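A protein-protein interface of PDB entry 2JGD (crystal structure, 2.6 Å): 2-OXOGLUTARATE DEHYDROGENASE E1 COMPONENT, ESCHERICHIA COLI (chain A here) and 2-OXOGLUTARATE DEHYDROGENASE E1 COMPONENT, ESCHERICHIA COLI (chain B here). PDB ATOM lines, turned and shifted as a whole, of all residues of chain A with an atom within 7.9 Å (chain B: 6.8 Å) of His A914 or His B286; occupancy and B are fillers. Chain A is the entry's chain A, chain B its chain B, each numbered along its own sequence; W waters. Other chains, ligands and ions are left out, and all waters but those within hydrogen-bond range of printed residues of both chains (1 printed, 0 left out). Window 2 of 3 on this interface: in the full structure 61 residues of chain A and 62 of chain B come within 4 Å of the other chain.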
ATOM      1  N   GLY A 724       5.179 -26.416  24.966  1.00  0.00           N
ATOM      2  CA  GLY A 724       4.986 -25.205  24.195  1.00  0.00           C
ATOM      3  C   GLY A 724       3.556 -24.697  24.082  1.00  0.00           C
ATOM      4  O   GLY A 724       3.270 -23.804  23.284  1.00  0.00           O
ATOM      5  N   GLN A 725       2.656 -25.204  24.901  1.00  0.00           N
ATOM      6  CA  GLN A 725       1.273 -24.710  24.871  1.00  0.00           C
ATOM      7  C   GLN A 725       0.953 -23.613  25.910  1.00  0.00           C
ATOM      8  O   GLN A 725      -0.218 -23.279  26.140  1.00  0.00           O
ATOM      9  CB  GLN A 725       0.313 -25.877  25.038  1.00  0.00           C
ATOM     10  CG  GLN A 725      -0.333 -26.312  23.759  1.00  0.00           C
ATOM     11  CD  GLN A 725      -0.382 -27.808  23.636  1.00  0.00           C
ATOM     12  OE1 GLN A 725      -0.990 -28.507  24.463  1.00  0.00           O
ATOM     13  NE2 GLN A 725       0.276 -28.323  22.611  1.00  0.00           N
ATOM     14  N   GLY A 726       1.981 -23.081  26.566  1.00  0.00           N
ATOM     15  CA  GLY A 726       1.806 -21.872  27.362  1.00  0.00           C
ATOM     16  C   GLY A 726       1.557 -22.081  28.848  1.00  0.00           C
ATOM     17  O   GLY A 726       1.443 -23.205  29.324  1.00  0.00           O
ATOM     18  N   PRO A 727       1.462 -20.977  29.583  1.00  0.00           N
ATOM     19  CA  PRO A 727       1.394 -20.906  31.033  1.00  0.00           C
ATOM     20  C   PRO A 727       0.344 -21.768  31.720  1.00  0.00           C
ATOM     21  O   PRO A 727       0.585 -22.215  32.832  1.00  0.00           O
ATOM     22  CB  PRO A 727       1.142 -19.418  31.303  1.00  0.00           C
ATOM     23  CG  PRO A 727       0.792 -18.824  29.965  1.00  0.00           C
ATOM     24  CD  PRO A 727       1.488 -19.639  28.970  1.00  0.00           C
ATOM     25  N   ALA A 911       5.365 -20.902  31.972  1.00  0.00           N
ATOM     26  CA  ALA A 911       5.723 -21.267  30.582  1.00  0.00           C
ATOM     27  C   ALA A 911       5.632 -20.079  29.644  1.00  0.00           C
ATOM     28  O   ALA A 911       4.681 -19.286  29.736  1.00  0.00           O
ATOM     29  CB  ALA A 911       4.817 -22.338  30.093  1.00  0.00           C
ATOM     30  N   VAL A 912       6.584 -19.977  28.717  1.00  0.00           N
ATOM     31  CA  VAL A 912       6.545 -18.873  27.729  1.00  0.00           C
ATOM     32  C   VAL A 912       5.324 -18.989  26.819  1.00  0.00           C
ATOM     33  O   VAL A 912       4.752 -20.077  26.639  1.00  0.00           O
ATOM     34  CB  VAL A 912       7.821 -18.800  26.838  1.00  0.00           C
ATOM     35  CG1 VAL A 912       9.060 -18.520  27.673  1.00  0.00           C
ATOM     36  CG2 VAL A 912       7.987 -20.084  26.058  1.00  0.00           C
ATOM     37  N   GLY A 913       4.918 -17.869  26.246  1.00  0.00           N
ATOM     38  CA  GLY A 913       3.741 -17.853  25.383  1.00  0.00           C
ATOM     39  C   GLY A 913       3.961 -18.526  24.031  1.00  0.00           C
ATOM     40  O   GLY A 913       3.017 -19.010  23.419  1.00  0.00           O
ATOM     41  N   HIS A 914       5.210 -18.576  23.571  1.00  0.00           N
ATOM     42  CA  HIS A 914       5.465 -18.693  22.137  1.00  0.00           C
ATOM     43  C   HIS A 914       6.239 -19.971  21.825  1.00  0.00           C
ATOM     44  O   HIS A 914       7.284 -20.254  22.425  1.00  0.00           O
ATOM     45  CB  HIS A 914       6.212 -17.451  21.600  1.00  0.00           C
ATOM     46  CG  HIS A 914       5.599 -16.130  21.993  1.00  0.00           C
ATOM     47  ND1 HIS A 914       6.354 -15.065  22.446  1.00  0.00           N
ATOM     48  CD2 HIS A 914       4.314 -15.694  21.975  1.00  0.00           C
ATOM     49  CE1 HIS A 914       5.560 -14.036  22.707  1.00  0.00           C
ATOM     50  NE2 HIS A 914       4.317 -14.390  22.428  1.00  0.00           N
ATOM     51  N   MET A 915       5.724 -20.756  20.890  1.00  0.00           N
ATOM     52  CA  MET A 915       6.253 -22.107  20.652  1.00  0.00           C
ATOM     53  C   MET A 915       7.745 -22.154  20.256  1.00  0.00           C
ATOM     54  O   MET A 915       8.485 -23.038  20.695  1.00  0.00           O
ATOM     55  CB  MET A 915       5.396 -22.846  19.621  1.00  0.00           C
ATOM     56  CG  MET A 915       6.004 -24.133  19.159  1.00  0.00           C
ATOM     57  SD  MET A 915       5.476 -25.512  20.189  1.00  0.00           S
ATOM     58  CE  MET A 915       6.908 -26.586  20.100  1.00  0.00           C
ATOM     59  N   SER A 916       8.188 -21.220  19.418  1.00  0.00           N
ATOM     60  CA  SER A 916       9.593 -21.218  18.994  1.00  0.00           C
ATOM     61  C   SER A 916      10.537 -20.988  20.178  1.00  0.00           C
ATOM     62  O   SER A 916      11.657 -21.527  20.209  1.00  0.00           O
ATOM     63  CB  SER A 916       9.855 -20.163  17.885  1.00  0.00           C
ATOM     64  OG  SER A 916       9.262 -18.911  18.204  1.00  0.00           O
ATOM     65  N   VAL A 917      10.106 -20.157  21.131  1.00  0.00           N
ATOM     66  CA  VAL A 917      10.911 -19.916  22.327  1.00  0.00           C
ATOM     67  C   VAL A 917      11.005 -21.174  23.193  1.00  0.00           C
ATOM     68  O   VAL A 917      12.099 -21.576  23.626  1.00  0.00           O
ATOM     69  CB  VAL A 917      10.391 -18.734  23.153  1.00  0.00           C
ATOM     70  CG1 VAL A 917      11.220 -18.598  24.435  1.00  0.00           C
ATOM     71  CG2 VAL A 917      10.484 -17.426  22.319  1.00  0.00           C
ATOM     72  N   HIS A 918       9.870 -21.829  23.399  1.00  0.00           N
ATOM     73  CA  HIS A 918       9.869 -23.126  24.078  1.00  0.00           C
ATOM     74  C   HIS A 918      10.895 -24.084  23.475  1.00  0.00           C
ATOM     75  O   HIS A 918      11.742 -24.628  24.188  1.00  0.00           O
ATOM     76  CB  HIS A 918       8.476 -23.744  24.043  1.00  0.00           C
ATOM     77  CG  HIS A 918       8.447 -25.186  24.427  1.00  0.00           C
ATOM     78  ND1 HIS A 918       8.607 -25.611  25.726  1.00  0.00           N
ATOM     79  CD2 HIS A 918       8.286 -26.304  23.680  1.00  0.00           C
ATOM     80  CE1 HIS A 918       8.527 -26.927  25.762  1.00  0.00           C
ATOM     81  NE2 HIS A 918       8.348 -27.372  24.531  1.00  0.00           N
ATOM     82  N   GLN A 919      10.831 -24.269  22.157  1.00  0.00           N
ATOM     83  CA  GLN A 919      11.663 -25.257  21.495  1.00  0.00           C
ATOM     84  C   GLN A 919      13.129 -24.991  21.699  1.00  0.00           C
ATOM     85  O   GLN A 919      13.897 -25.907  21.987  1.00  0.00           O
ATOM     86  CB  GLN A 919      11.360 -25.306  20.019  1.00  0.00           C
ATOM     87  CG  GLN A 919      10.097 -26.095  19.691  1.00  0.00           C
ATOM     88  CD  GLN A 919       9.590 -25.791  18.285  1.00  0.00           C
ATOM     89  OE1 GLN A 919       8.727 -26.487  17.759  1.00  0.00           O
ATOM     90  NE2 GLN A 919      10.133 -24.735  17.672  1.00  0.00           N
ATOM     91  N   LYS A 920      13.523 -23.732  21.566  1.00  0.00           N
ATOM     92  CA  LYS A 920      14.898 -23.348  21.876  1.00  0.00           C
ATOM     93  C   LYS A 920      15.285 -23.704  23.306  1.00  0.00           C
ATOM     94  O   LYS A 920      16.360 -24.293  23.537  1.00  0.00           O
ATOM     95  CB  LYS A 920      15.140 -21.862  21.597  1.00  0.00           C
ATOM     96  CG  LYS A 920      16.488 -21.342  22.060  1.00  0.00           C
ATOM     97  CD  LYS A 920      17.523 -21.415  20.949  1.00  0.00           C
ATOM     98  CE  LYS A 920      18.364 -20.151  20.908  1.00  0.00           C
ATOM     99  NZ  LYS A 920      19.419 -20.158  21.959  1.00  0.00           N
ATOM    100  N   GLN A 921      14.406 -23.407  24.267  1.00  0.00           N
ATOM    101  CA  GLN A 921      14.716 -23.736  25.676  1.00  0.00           C
ATOM    102  C   GLN A 921      14.896 -25.258  25.905  1.00  0.00           C
ATOM    103  O   GLN A 921      15.822 -25.692  26.604  1.00  0.00           O
ATOM    104  CB  GLN A 921      13.655 -23.185  26.616  1.00  0.00           C
ATOM    105  CG  GLN A 921      13.494 -21.666  26.618  1.00  0.00           C
ATOM    106  CD  GLN A 921      12.309 -21.224  27.485  1.00  0.00           C
ATOM    107  OE1 GLN A 921      11.258 -21.876  27.496  1.00  0.00           O
ATOM    108  NE2 GLN A 921      12.479 -20.123  28.222  1.00  0.00           N
ATOM    109  N   ASP B 280       0.150 -11.808  11.686  1.00  0.00           N
ATOM    110  CA  ASP B 280       1.511 -11.979  12.159  1.00  0.00           C
ATOM    111  C   ASP B 280       1.545 -12.935  13.349  1.00  0.00           C
ATOM    112  O   ASP B 280       2.367 -13.846  13.400  1.00  0.00           O
ATOM    113  CB  ASP B 280       2.125 -10.630  12.522  1.00  0.00           C
ATOM    114  CG  ASP B 280       2.386  -9.760  11.299  1.00  0.00           C
ATOM    115  OD1 ASP B 280       2.202 -10.257  10.160  1.00  0.00           O
ATOM    116  OD2 ASP B 280       2.780  -8.580  11.478  1.00  0.00           O
ATOM    117  N   GLU B 281       0.618 -12.754  14.286  1.00  0.00           N
ATOM    118  CA  GLU B 281       0.612 -13.566  15.492  1.00  0.00           C
ATOM    119  C   GLU B 281       0.491 -15.039  15.158  1.00  0.00           C
ATOM    120  O   GLU B 281       1.184 -15.867  15.744  1.00  0.00           O
ATOM    121  CB  GLU B 281      -0.501 -13.146  16.445  1.00  0.00           C
ATOM    122  CG  GLU B 281      -0.093 -12.081  17.464  1.00  0.00           C
ATOM    123  CD  GLU B 281      -1.286 -11.407  18.128  1.00  0.00           C
ATOM    124  OE1 GLU B 281      -1.259 -10.165  18.293  1.00  0.00           O
ATOM    125  OE2 GLU B 281      -2.258 -12.117  18.471  1.00  0.00           O
ATOM    126  N   PHE B 282      -0.388 -15.370  14.217  1.00  0.00           N
ATOM    127  CA  PHE B 282      -0.535 -16.764  13.779  1.00  0.00           C
ATOM    128  C   PHE B 282       0.738 -17.269  13.135  1.00  0.00           C
ATOM    129  O   PHE B 282       0.950 -18.481  13.034  1.00  0.00           O
ATOM    130  CB  PHE B 282      -1.664 -16.907  12.772  1.00  0.00           C
ATOM    131  CG  PHE B 282      -3.017 -17.031  13.389  1.00  0.00           C
ATOM    132  CD1 PHE B 282      -3.854 -15.937  13.468  1.00  0.00           C
ATOM    133  CD2 PHE B 282      -3.469 -18.251  13.857  1.00  0.00           C
ATOM    134  CE1 PHE B 282      -5.117 -16.062  14.003  1.00  0.00           C
ATOM    135  CE2 PHE B 282      -4.729 -18.377  14.383  1.00  0.00           C
ATOM    136  CZ  PHE B 282      -5.554 -17.280  14.459  1.00  0.00           C
ATOM    137  N   ALA B 283       1.579 -16.338  12.687  1.00  0.00           N
ATOM    138  CA  ALA B 283       2.826 -16.688  12.013  1.00  0.00           C
ATOM    139  C   ALA B 283       4.045 -16.643  12.953  1.00  0.00           C
ATOM    140  O   ALA B 283       5.178 -16.873  12.526  1.00  0.00           O
ATOM    141  CB  ALA B 283       3.040 -15.776  10.806  1.00  0.00           C
ATOM    142  N   GLY B 284       3.808 -16.333  14.226  1.00  0.00           N
ATOM    143  CA  GLY B 284       4.862 -16.365  15.238  1.00  0.00           C
ATOM    144  C   GLY B 284       5.879 -15.244  15.112  1.00  0.00           C
ATOM    145  O   GLY B 284       6.940 -15.283  15.739  1.00  0.00           O
ATOM    146  N   LYS B 285       5.564 -14.245  14.293  1.00  0.00           N
ATOM    147  CA  LYS B 285       6.258 -12.964  14.358  1.00  0.00           C
ATOM    148  C   LYS B 285       5.659 -12.142  15.487  1.00  0.00           C
ATOM    149  O   LYS B 285       4.477 -11.795  15.446  1.00  0.00           O
ATOM    150  CB  LYS B 285       6.113 -12.206  13.039  1.00  0.00           C
ATOM    151  CG  LYS B 285       6.536 -12.996  11.812  1.00  0.00           C
ATOM    152  N   HIS B 286       6.461 -11.846  16.508  1.00  0.00           N
ATOM    153  CA  HIS B 286       5.903 -11.278  17.735  1.00  0.00           C
ATOM    154  C   HIS B 286       6.370  -9.873  18.097  1.00  0.00           C
ATOM    155  O   HIS B 286       7.558  -9.548  17.985  1.00  0.00           O
ATOM    156  CB  HIS B 286       6.042 -12.239  18.912  1.00  0.00           C
ATOM    157  CG  HIS B 286       4.983 -13.294  18.941  1.00  0.00           C
ATOM    158  ND1 HIS B 286       5.228 -14.607  18.597  1.00  0.00           N
ATOM    159  CD2 HIS B 286       3.659 -13.217  19.214  1.00  0.00           C
ATOM    160  CE1 HIS B 286       4.105 -15.298  18.677  1.00  0.00           C
ATOM    161  NE2 HIS B 286       3.138 -14.478  19.047  1.00  0.00           N
ATOM    162  N   GLY B 291       8.557  -9.395  27.508  1.00  0.00           N
ATOM    163  CA  GLY B 291       8.360 -10.455  28.490  1.00  0.00           C
ATOM    164  C   GLY B 291       8.092 -11.800  27.848  1.00  0.00           C
ATOM    165  O   GLY B 291       8.324 -11.981  26.665  1.00  0.00           O
ATOM    166  N   THR B 292       7.593 -12.749  28.627  1.00  0.00           N
ATOM    167  CA  THR B 292       7.471 -14.140  28.155  1.00  0.00           C
ATOM    168  C   THR B 292       6.174 -14.469  27.401  1.00  0.00           C
ATOM    169  O   THR B 292       6.095 -15.488  26.727  1.00  0.00           O
ATOM    170  CB  THR B 292       7.631 -15.127  29.300  1.00  0.00           C
ATOM    171  OG1 THR B 292       6.673 -14.819  30.321  1.00  0.00           O
ATOM    172  CG2 THR B 292       9.027 -15.012  29.883  1.00  0.00           C
ATOM    173  N   GLY B 293       5.164 -13.619  27.537  1.00  0.00           N
ATOM    174  CA  GLY B 293       4.020 -13.631  26.637  1.00  0.00           C
ATOM    175  C   GLY B 293       2.947 -14.664  26.935  1.00  0.00           C
ATOM    176  O   GLY B 293       2.974 -15.343  27.956  1.00  0.00           O
ATOM    177  N   ASP B 294       1.988 -14.783  26.034  1.00  0.00           N
ATOM    178  CA  ASP B 294       0.861 -15.653  26.283  1.00  0.00           C
ATOM    179  C   ASP B 294       0.092 -15.832  24.985  1.00  0.00           C
ATOM    180  O   ASP B 294       0.445 -15.242  23.984  1.00  0.00           O
ATOM    181  CB  ASP B 294      -0.024 -15.053  27.368  1.00  0.00           C
ATOM    182  CG  ASP B 294      -1.056 -16.046  27.905  1.00  0.00           C
ATOM    183  OD1 ASP B 294      -0.975 -17.257  27.573  1.00  0.00           O
ATOM    184  OD2 ASP B 294      -1.956 -15.612  28.660  1.00  0.00           O
ATOM    185  N   VAL B 295      -0.935 -16.669  24.985  1.00  0.00           N
ATOM    186  CA  VAL B 295      -1.549 -17.089  23.731  1.00  0.00           C
ATOM    187  C   VAL B 295      -2.533 -16.027  23.256  1.00  0.00           C
ATOM    188  O   VAL B 295      -3.083 -15.285  24.062  1.00  0.00           O
ATOM    189  CB  VAL B 295      -2.260 -18.430  23.904  1.00  0.00           C
ATOM    190  CG1 VAL B 295      -1.255 -19.479  24.293  1.00  0.00           C
ATOM    191  CG2 VAL B 295      -3.333 -18.326  25.001  1.00  0.00           C
ATOM    192  N   LYS B 296      -2.738 -15.942  21.949  1.00  0.00           N
ATOM    193  CA  LYS B 296      -3.455 -14.813  21.367  1.00  0.00           C
ATOM    194  C   LYS B 296      -4.878 -14.713  21.903  1.00  0.00           C
ATOM    195  O   LYS B 296      -5.468 -13.638  21.921  1.00  0.00           O
ATOM    196  CB  LYS B 296      -3.501 -14.928  19.853  1.00  0.00           C
ATOM    197  CG  LYS B 296      -4.303 -16.146  19.332  1.00  0.00           C
ATOM    198  CD  LYS B 296      -4.076 -16.370  17.817  1.00  0.00           C
ATOM    199  CE  LYS B 296      -2.826 -17.220  17.545  1.00  0.00           C
ATOM    200  NZ  LYS B 296      -3.203 -18.660  17.339  1.00  0.00           N
HETATM  201  O   HOH W   1       4.644 -16.469  29.806  1.00  0.00           O
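The backbone NH of Gly A913 lies within hydrogen-bond range of the backbone carbonyl oxygen of Thr B292.
O of Gly B284 lies within hydrogen-bond range of ND1 of His B286 (3.4 Å).
Among the printed residues, merely in contact across the chains: Pro A727 with Asp B294 (3.4 Å), Val A912 with Thr B292 (3.6 Å), Gly A913 with Gly B293 (3.6 Å), Gly A913 with Asp B294 (3.6 Å) and His A914 with His B286 (3.3 Å).
Printed residues of chain B within 4 Å of Pro A727: Asp B294 (3.4 Å).
Printed residues of chain B within 4 Å of Gly A913: Thr B292, Gly B293 and Asp B294.
His A914 touches just one residue of chain B: His B286 (3.3 Å).
His B286 touches just one residue of chain A: His A914 (3.3 Å).
Of the printed residues of chain A, Asp B294 touches Pro A727 and Gly A913.
The nearest printed residue of chain B that does not touch His A914 is Gly B293 (4.2 Å).
Of the 15 printed residues of chain A, 4 touch a printed residue of chain B.
Hydrophobic or aromatic side chains of chain A within 4 Å of the printed part of chain B: Pro A727, Val A912 and His A914.
Among the printed residues, no Asp or Glu carboxylate lies within 4 Å of a Lys or Arg side-chain nitrogen of the other chain.
Water W1 lies within hydrogen-bond range of OG1 of Thr B292, O of Gly B293 and O of Ala A911.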
